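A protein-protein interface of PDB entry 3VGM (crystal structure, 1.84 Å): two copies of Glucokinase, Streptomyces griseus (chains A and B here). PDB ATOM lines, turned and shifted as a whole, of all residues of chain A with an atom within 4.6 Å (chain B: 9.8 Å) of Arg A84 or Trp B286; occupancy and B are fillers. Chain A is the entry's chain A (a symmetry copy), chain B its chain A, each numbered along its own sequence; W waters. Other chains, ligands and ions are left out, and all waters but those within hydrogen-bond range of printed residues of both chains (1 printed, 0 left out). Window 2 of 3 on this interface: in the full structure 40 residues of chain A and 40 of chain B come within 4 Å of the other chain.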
ATOM      1  N   VAL A  75     -20.332 -20.180  24.892  1.00  0.00           N
ATOM      2  CA  VAL A  75     -20.858 -21.006  25.971  1.00  0.00           C
ATOM      3  C   VAL A  75     -21.594 -22.159  25.292  1.00  0.00           C
ATOM      4  O   VAL A  75     -22.643 -21.967  24.651  1.00  0.00           O
ATOM      5  CB  VAL A  75     -21.820 -20.248  26.931  1.00  0.00           C
ATOM      6  CG1 VAL A  75     -22.352 -21.218  27.993  1.00  0.00           C
ATOM      7  CG2 VAL A  75     -21.109 -19.033  27.618  1.00  0.00           C
ATOM      8  N   LEU A  76     -21.033 -23.359  25.409  1.00  0.00           N
ATOM      9  CA  LEU A  76     -21.598 -24.520  24.738  1.00  0.00           C
ATOM     10  C   LEU A  76     -22.894 -24.932  25.401  1.00  0.00           C
ATOM     11  O   LEU A  76     -23.837 -25.338  24.720  1.00  0.00           O
ATOM     12  CB  LEU A  76     -20.614 -25.703  24.752  1.00  0.00           C
ATOM     13  CG  LEU A  76     -19.280 -25.404  24.074  1.00  0.00           C
ATOM     14  CD1 LEU A  76     -18.318 -26.610  24.368  1.00  0.00           C
ATOM     15  CD2 LEU A  76     -19.462 -25.191  22.571  1.00  0.00           C
ATOM     16  N   PHE A  77     -22.921 -24.842  26.731  1.00  0.00           N
ATOM     17  CA  PHE A  77     -24.085 -25.197  27.526  1.00  0.00           C
ATOM     18  C   PHE A  77     -23.976 -24.469  28.855  1.00  0.00           C
ATOM     19  O   PHE A  77     -22.929 -24.496  29.480  1.00  0.00           O
ATOM     20  CB  PHE A  77     -24.108 -26.713  27.784  1.00  0.00           C
ATOM     21  CG  PHE A  77     -25.147 -27.172  28.799  1.00  0.00           C
ATOM     22  CD1 PHE A  77     -26.423 -27.543  28.389  1.00  0.00           C
ATOM     23  CD2 PHE A  77     -24.825 -27.271  30.153  1.00  0.00           C
ATOM     24  CE1 PHE A  77     -27.390 -27.974  29.319  1.00  0.00           C
ATOM     25  CE2 PHE A  77     -25.767 -27.706  31.093  1.00  0.00           C
ATOM     26  CZ  PHE A  77     -27.053 -28.061  30.679  1.00  0.00           C
ATOM     27  N   ALA A  78     -25.063 -23.844  29.295  1.00  0.00           N
ATOM     28  CA  ALA A  78     -25.121 -23.275  30.651  1.00  0.00           C
ATOM     29  C   ALA A  78     -26.238 -23.952  31.455  1.00  0.00           C
ATOM     30  O   ALA A  78     -27.342 -24.133  30.942  1.00  0.00           O
ATOM     31  CB  ALA A  78     -25.355 -21.765  30.585  1.00  0.00           C
ATOM     32  N   ILE A  81     -28.995 -20.923  32.270  1.00  0.00           N
ATOM     33  CA  ILE A  81     -29.355 -19.966  31.219  1.00  0.00           C
ATOM     34  C   ILE A  81     -29.613 -20.770  29.954  1.00  0.00           C
ATOM     35  O   ILE A  81     -28.927 -21.764  29.694  1.00  0.00           O
ATOM     36  CB  ILE A  81     -28.230 -18.930  30.970  1.00  0.00           C
ATOM     37  CG1 ILE A  81     -27.872 -18.210  32.282  1.00  0.00           C
ATOM     38  CG2 ILE A  81     -28.623 -17.939  29.869  1.00  0.00           C
ATOM     39  CD1 ILE A  81     -26.555 -17.419  32.257  1.00  0.00           C
ATOM     40  N   ASP A  82     -30.601 -20.353  29.166  1.00  0.00           N
ATOM     41  CA  ASP A  82     -30.890 -21.059  27.918  1.00  0.00           C
ATOM     42  C   ASP A  82     -29.872 -20.632  26.853  1.00  0.00           C
ATOM     43  O   ASP A  82     -30.207 -19.969  25.847  1.00  0.00           O
ATOM     44  CB  ASP A  82     -32.343 -20.813  27.466  1.00  0.00           C
ATOM     45  CG  ASP A  82     -32.762 -21.718  26.312  1.00  0.00           C
ATOM     46  OD1 ASP A  82     -33.644 -21.296  25.534  1.00  0.00           O
ATOM     47  OD2 ASP A  82     -32.205 -22.842  26.175  1.00  0.00           O
ATOM     48  N   TRP A  83     -28.613 -20.980  27.108  1.00  0.00           N
ATOM     49  CA  TRP A  83     -27.527 -20.754  26.164  1.00  0.00           C
ATOM     50  C   TRP A  83     -27.057 -22.107  25.681  1.00  0.00           C
ATOM     51  O   TRP A  83     -26.749 -22.998  26.495  1.00  0.00           O
ATOM     52  CB  TRP A  83     -26.353 -20.042  26.832  1.00  0.00           C
ATOM     53  CG  TRP A  83     -26.487 -18.552  26.938  1.00  0.00           C
ATOM     54  CD1 TRP A  83     -27.341 -17.737  26.240  1.00  0.00           C
ATOM     55  CD2 TRP A  83     -25.713 -17.698  27.784  1.00  0.00           C
ATOM     56  NE1 TRP A  83     -27.148 -16.421  26.611  1.00  0.00           N
ATOM     57  CE2 TRP A  83     -26.158 -16.370  27.560  1.00  0.00           C
ATOM     58  CE3 TRP A  83     -24.691 -17.930  28.719  1.00  0.00           C
ATOM     59  CZ2 TRP A  83     -25.611 -15.265  28.232  1.00  0.00           C
ATOM     60  CZ3 TRP A  83     -24.145 -16.835  29.399  1.00  0.00           C
ATOM     61  CH2 TRP A  83     -24.610 -15.515  29.146  1.00  0.00           C
ATOM     62  N   ARG A  84     -27.028 -22.262  24.365  1.00  0.00           N
ATOM     63  CA  ARG A  84     -26.572 -23.495  23.729  1.00  0.00           C
ATOM     64  C   ARG A  84     -25.770 -23.019  22.534  1.00  0.00           C
ATOM     65  O   ARG A  84     -26.323 -22.359  21.627  1.00  0.00           O
ATOM     66  CB  ARG A  84     -27.750 -24.370  23.277  1.00  0.00           C
ATOM     67  CG  ARG A  84     -28.738 -24.795  24.364  1.00  0.00           C
ATOM     68  CD  ARG A  84     -28.119 -25.750  25.399  1.00  0.00           C
ATOM     69  NE  ARG A  84     -29.084 -26.136  26.422  1.00  0.00           N
ATOM     70  CZ  ARG A  84     -29.233 -25.517  27.590  1.00  0.00           C
ATOM     71  NH1 ARG A  84     -28.467 -24.476  27.915  1.00  0.00           N
ATOM     72  NH2 ARG A  84     -30.145 -25.946  28.448  1.00  0.00           N
ATOM     73  N   HIS A  85     -24.467 -23.287  22.556  1.00  0.00           N
ATOM     74  CA  HIS A  85     -23.550 -22.742  21.543  1.00  0.00           C
ATOM     75  C   HIS A  85     -23.758 -21.234  21.365  1.00  0.00           C
ATOM     76  O   HIS A  85     -23.855 -20.739  20.232  1.00  0.00           O
ATOM     77  CB  HIS A  85     -23.720 -23.470  20.199  1.00  0.00           C
ATOM     78  CG  HIS A  85     -23.549 -24.953  20.294  1.00  0.00           C
ATOM     79  ND1 HIS A  85     -22.312 -25.555  20.365  1.00  0.00           N
ATOM     80  CD2 HIS A  85     -24.461 -25.961  20.308  1.00  0.00           C
ATOM     81  CE1 HIS A  85     -22.464 -26.868  20.448  1.00  0.00           C
ATOM     82  NE2 HIS A  85     -23.759 -27.142  20.401  1.00  0.00           N
ATOM     83  N   GLU A  86     -23.816 -20.523  22.495  1.00  0.00           N
ATOM     84  CA  GLU A  86     -24.063 -19.082  22.509  1.00  0.00           C
ATOM     85  C   GLU A  86     -22.772 -18.328  22.240  1.00  0.00           C
ATOM     86  O   GLU A  86     -21.825 -18.468  23.009  1.00  0.00           O
ATOM     87  CB  GLU A  86     -24.625 -18.675  23.872  1.00  0.00           C
ATOM     88  CG  GLU A  86     -24.840 -17.148  24.024  1.00  0.00           C
ATOM     89  CD  GLU A  86     -26.008 -16.638  23.194  1.00  0.00           C
ATOM     90  OE1 GLU A  86     -26.755 -17.472  22.608  1.00  0.00           O
ATOM     91  OE2 GLU A  86     -26.176 -15.396  23.139  1.00  0.00           O
ATOM     92  N   ASP B 252     -10.642 -33.415  29.941  1.00  0.00           N
ATOM     93  CA  ASP B 252     -11.127 -33.044  28.593  1.00  0.00           C
ATOM     94  C   ASP B 252     -10.042 -33.197  27.501  1.00  0.00           C
ATOM     95  O   ASP B 252      -9.753 -32.242  26.789  1.00  0.00           O
ATOM     96  CB  ASP B 252     -11.665 -31.604  28.599  1.00  0.00           C
ATOM     97  CG  ASP B 252     -12.405 -31.239  27.300  1.00  0.00           C
ATOM     98  OD1 ASP B 252     -13.149 -32.101  26.768  1.00  0.00           O
ATOM     99  OD2 ASP B 252     -12.269 -30.081  26.842  1.00  0.00           O
ATOM    100  N   LEU B 281     -20.792 -39.798  29.249  1.00  0.00           N
ATOM    101  CA  LEU B 281     -20.123 -38.517  29.009  1.00  0.00           C
ATOM    102  C   LEU B 281     -21.069 -37.350  29.323  1.00  0.00           C
ATOM    103  O   LEU B 281     -22.089 -37.167  28.662  1.00  0.00           O
ATOM    104  CB  LEU B 281     -19.632 -38.423  27.548  1.00  0.00           C
ATOM    105  CG  LEU B 281     -18.952 -37.090  27.161  1.00  0.00           C
ATOM    106  CD1 LEU B 281     -17.671 -36.840  28.015  1.00  0.00           C
ATOM    107  CD2 LEU B 281     -18.655 -37.041  25.658  1.00  0.00           C
ATOM    108  N   ILE B 282     -20.741 -36.563  30.339  1.00  0.00           N
ATOM    109  CA  ILE B 282     -21.691 -35.508  30.744  1.00  0.00           C
ATOM    110  C   ILE B 282     -21.618 -34.378  29.738  1.00  0.00           C
ATOM    111  O   ILE B 282     -20.525 -34.026  29.248  1.00  0.00           O
ATOM    112  CB  ILE B 282     -21.482 -35.033  32.216  1.00  0.00           C
ATOM    113  CG1 ILE B 282     -20.166 -34.282  32.378  1.00  0.00           C
ATOM    114  CG2 ILE B 282     -21.556 -36.229  33.234  1.00  0.00           C
ATOM    115  CD1 ILE B 282     -20.376 -32.715  32.335  1.00  0.00           C
ATOM    116  N   GLY B 283     -22.781 -33.830  29.388  1.00  0.00           N
ATOM    117  CA  GLY B 283     -22.832 -32.766  28.394  1.00  0.00           C
ATOM    118  C   GLY B 283     -22.487 -33.230  26.989  1.00  0.00           C
ATOM    119  O   GLY B 283     -22.161 -32.419  26.121  1.00  0.00           O
ATOM    120  N   GLY B 284     -22.582 -34.538  26.749  1.00  0.00           N
ATOM    121  CA  GLY B 284     -22.212 -35.135  25.447  1.00  0.00           C
ATOM    122  C   GLY B 284     -22.994 -34.591  24.255  1.00  0.00           C
ATOM    123  O   GLY B 284     -22.520 -34.644  23.113  1.00  0.00           O
ATOM    124  N   GLU B 285     -24.187 -34.058  24.513  1.00  0.00           N
ATOM    125  CA  GLU B 285     -24.961 -33.417  23.460  1.00  0.00           C
ATOM    126  C   GLU B 285     -24.306 -32.098  22.959  1.00  0.00           C
ATOM    127  O   GLU B 285     -24.483 -31.701  21.798  1.00  0.00           O
ATOM    128  CB  GLU B 285     -26.391 -33.169  23.941  1.00  0.00           C
ATOM    129  CG  GLU B 285     -27.285 -32.532  22.890  1.00  0.00           C
ATOM    130  CD  GLU B 285     -28.750 -32.534  23.257  1.00  0.00           C
ATOM    131  OE1 GLU B 285     -29.106 -32.847  24.421  1.00  0.00           O
ATOM    132  OE2 GLU B 285     -29.545 -32.203  22.364  1.00  0.00           O
ATOM    133  N   TRP B 286     -23.552 -31.436  23.841  1.00  0.00           N
ATOM    134  CA  TRP B 286     -23.111 -30.047  23.614  1.00  0.00           C
ATOM    135  C   TRP B 286     -21.611 -29.872  23.406  1.00  0.00           C
ATOM    136  O   TRP B 286     -21.177 -28.822  22.915  1.00  0.00           O
ATOM    137  CB  TRP B 286     -23.550 -29.199  24.818  1.00  0.00           C
ATOM    138  CG  TRP B 286     -24.954 -29.458  25.187  1.00  0.00           C
ATOM    139  CD1 TRP B 286     -25.425 -30.095  26.314  1.00  0.00           C
ATOM    140  CD2 TRP B 286     -26.100 -29.097  24.414  1.00  0.00           C
ATOM    141  NE1 TRP B 286     -26.806 -30.124  26.286  1.00  0.00           N
ATOM    142  CE2 TRP B 286     -27.241 -29.534  25.125  1.00  0.00           C
ATOM    143  CE3 TRP B 286     -26.269 -28.453  23.173  1.00  0.00           C
ATOM    144  CZ2 TRP B 286     -28.548 -29.343  24.643  1.00  0.00           C
ATOM    145  CZ3 TRP B 286     -27.569 -28.257  22.691  1.00  0.00           C
ATOM    146  CH2 TRP B 286     -28.694 -28.707  23.433  1.00  0.00           C
ATOM    147  N   ARG B 287     -20.825 -30.857  23.834  1.00  0.00           N
ATOM    148  CA  ARG B 287     -19.375 -30.743  23.824  1.00  0.00           C
ATOM    149  C   ARG B 287     -18.796 -31.750  22.820  1.00  0.00           C
ATOM    150  O   ARG B 287     -19.422 -32.791  22.559  1.00  0.00           O
ATOM    151  CB  ARG B 287     -18.821 -31.042  25.240  1.00  0.00           C
ATOM    152  CG  ARG B 287     -18.818 -32.568  25.550  1.00  0.00           C
ATOM    153  CD  ARG B 287     -18.637 -32.911  26.982  1.00  0.00           C
ATOM    154  NE  ARG B 287     -17.235 -32.812  27.358  1.00  0.00           N
ATOM    155  CZ  ARG B 287     -16.770 -33.101  28.557  1.00  0.00           C
ATOM    156  NH1 ARG B 287     -15.463 -32.959  28.791  1.00  0.00           N
ATOM    157  NH2 ARG B 287     -17.606 -33.515  29.525  1.00  0.00           N
ATOM    158  N   PRO B 288     -17.582 -31.478  22.295  1.00  0.00           N
ATOM    159  CA  PRO B 288     -16.925 -32.490  21.442  1.00  0.00           C
ATOM    160  C   PRO B 288     -16.545 -33.755  22.224  1.00  0.00           C
ATOM    161  O   PRO B 288     -16.236 -33.677  23.417  1.00  0.00           O
ATOM    162  CB  PRO B 288     -15.675 -31.774  20.937  1.00  0.00           C
ATOM    163  CG  PRO B 288     -16.053 -30.273  20.992  1.00  0.00           C
ATOM    164  CD  PRO B 288     -16.855 -30.192  22.285  1.00  0.00           C
ATOM    165  N   HIS B 289     -16.591 -34.908  21.561  1.00  0.00           N
ATOM    166  CA  HIS B 289     -16.222 -36.168  22.198  1.00  0.00           C
ATOM    167  C   HIS B 289     -14.766 -36.496  21.952  1.00  0.00           C
ATOM    168  O   HIS B 289     -14.312 -36.528  20.793  1.00  0.00           O
ATOM    169  CB  HIS B 289     -17.038 -37.316  21.617  1.00  0.00           C
ATOM    170  CG  HIS B 289     -18.499 -37.228  21.906  1.00  0.00           C
ATOM    171  ND1 HIS B 289     -19.308 -38.341  21.938  1.00  0.00           N
ATOM    172  CD2 HIS B 289     -19.292 -36.169  22.208  1.00  0.00           C
ATOM    173  CE1 HIS B 289     -20.549 -37.966  22.203  1.00  0.00           C
ATOM    174  NE2 HIS B 289     -20.563 -36.656  22.381  1.00  0.00           N
HETATM  175  O   HOH W   1     -24.595 -29.655  20.128  1.00  0.00           O
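Among the printed residues, merely in contact across the chains: Phe A77 with Trp B286 (3.4 Å), His A85 with Trp B286 (3.4 Å), Arg A84 with Trp B286 (3.6 Å) and Leu A76 with Trp B286 (3.7 Å).
Of chain B, only Trp B286 (3.7 Å) comes within 4 Å of Leu A76.
Of the printed residues of chain B, Phe A77 touches Trp B286 (3.4 Å).
Of chain B, only Trp B286 comes within 4 Å of Arg A84.
His A85 touches just one residue of chain B: Trp B286.
Gly B283 touches none of the printed residues of chain A.
The nearest residue of chain B that does not touch Arg A84 is Glu B285 (7.0 Å).
The nearest printed residue of chain A that does not touch Trp B286 is Trp A83 (6.4 Å).
The nearest printed residue of chain B that does not touch Phe A77 is Gly B283 (6.1 Å).
The backbone carbonyl oxygen (O) of Val A75 lies within hydrogen-bond range of the backbone NH (N) of His A85.
The backbone carbonyl oxygen (O) of Leu A76 lies within hydrogen-bond range of the backbone NH (N) of His A85.
O of Ala A78 sits at hydrogen-bond distance from NH1 of Arg A84, 3.2 Å away.
The backbone carbonyl oxygen (O) of Ile A81 is in hydrogen-bond range of the guanidinium group (NH1) of Arg A84 (3.3 Å).
Water W1 lies within hydrogen-bond range of the backbone carbonyl oxygen (O) of Glu B285 (2.6 Å) and a ring nitrogen (NE2) of His A85 (2.7 Å).
Of the 10 printed residues of chain A, 4 touch a printed residue of chain B.
Hydrophobic or aromatic side chains of chain A that line the printed part of chain B: Leu A76, Phe A77 and His A85.
Along chain A the printed residues that touch a printed residue of chain B span positions 76 to 85.
Printed residues of chain B that touch a printed residue of chain A: Trp B286.
No position is printed for both chains.
Of the 4 pairs that touch across the chains among the printed residues, none has its exchanged pair printed and touching as well.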
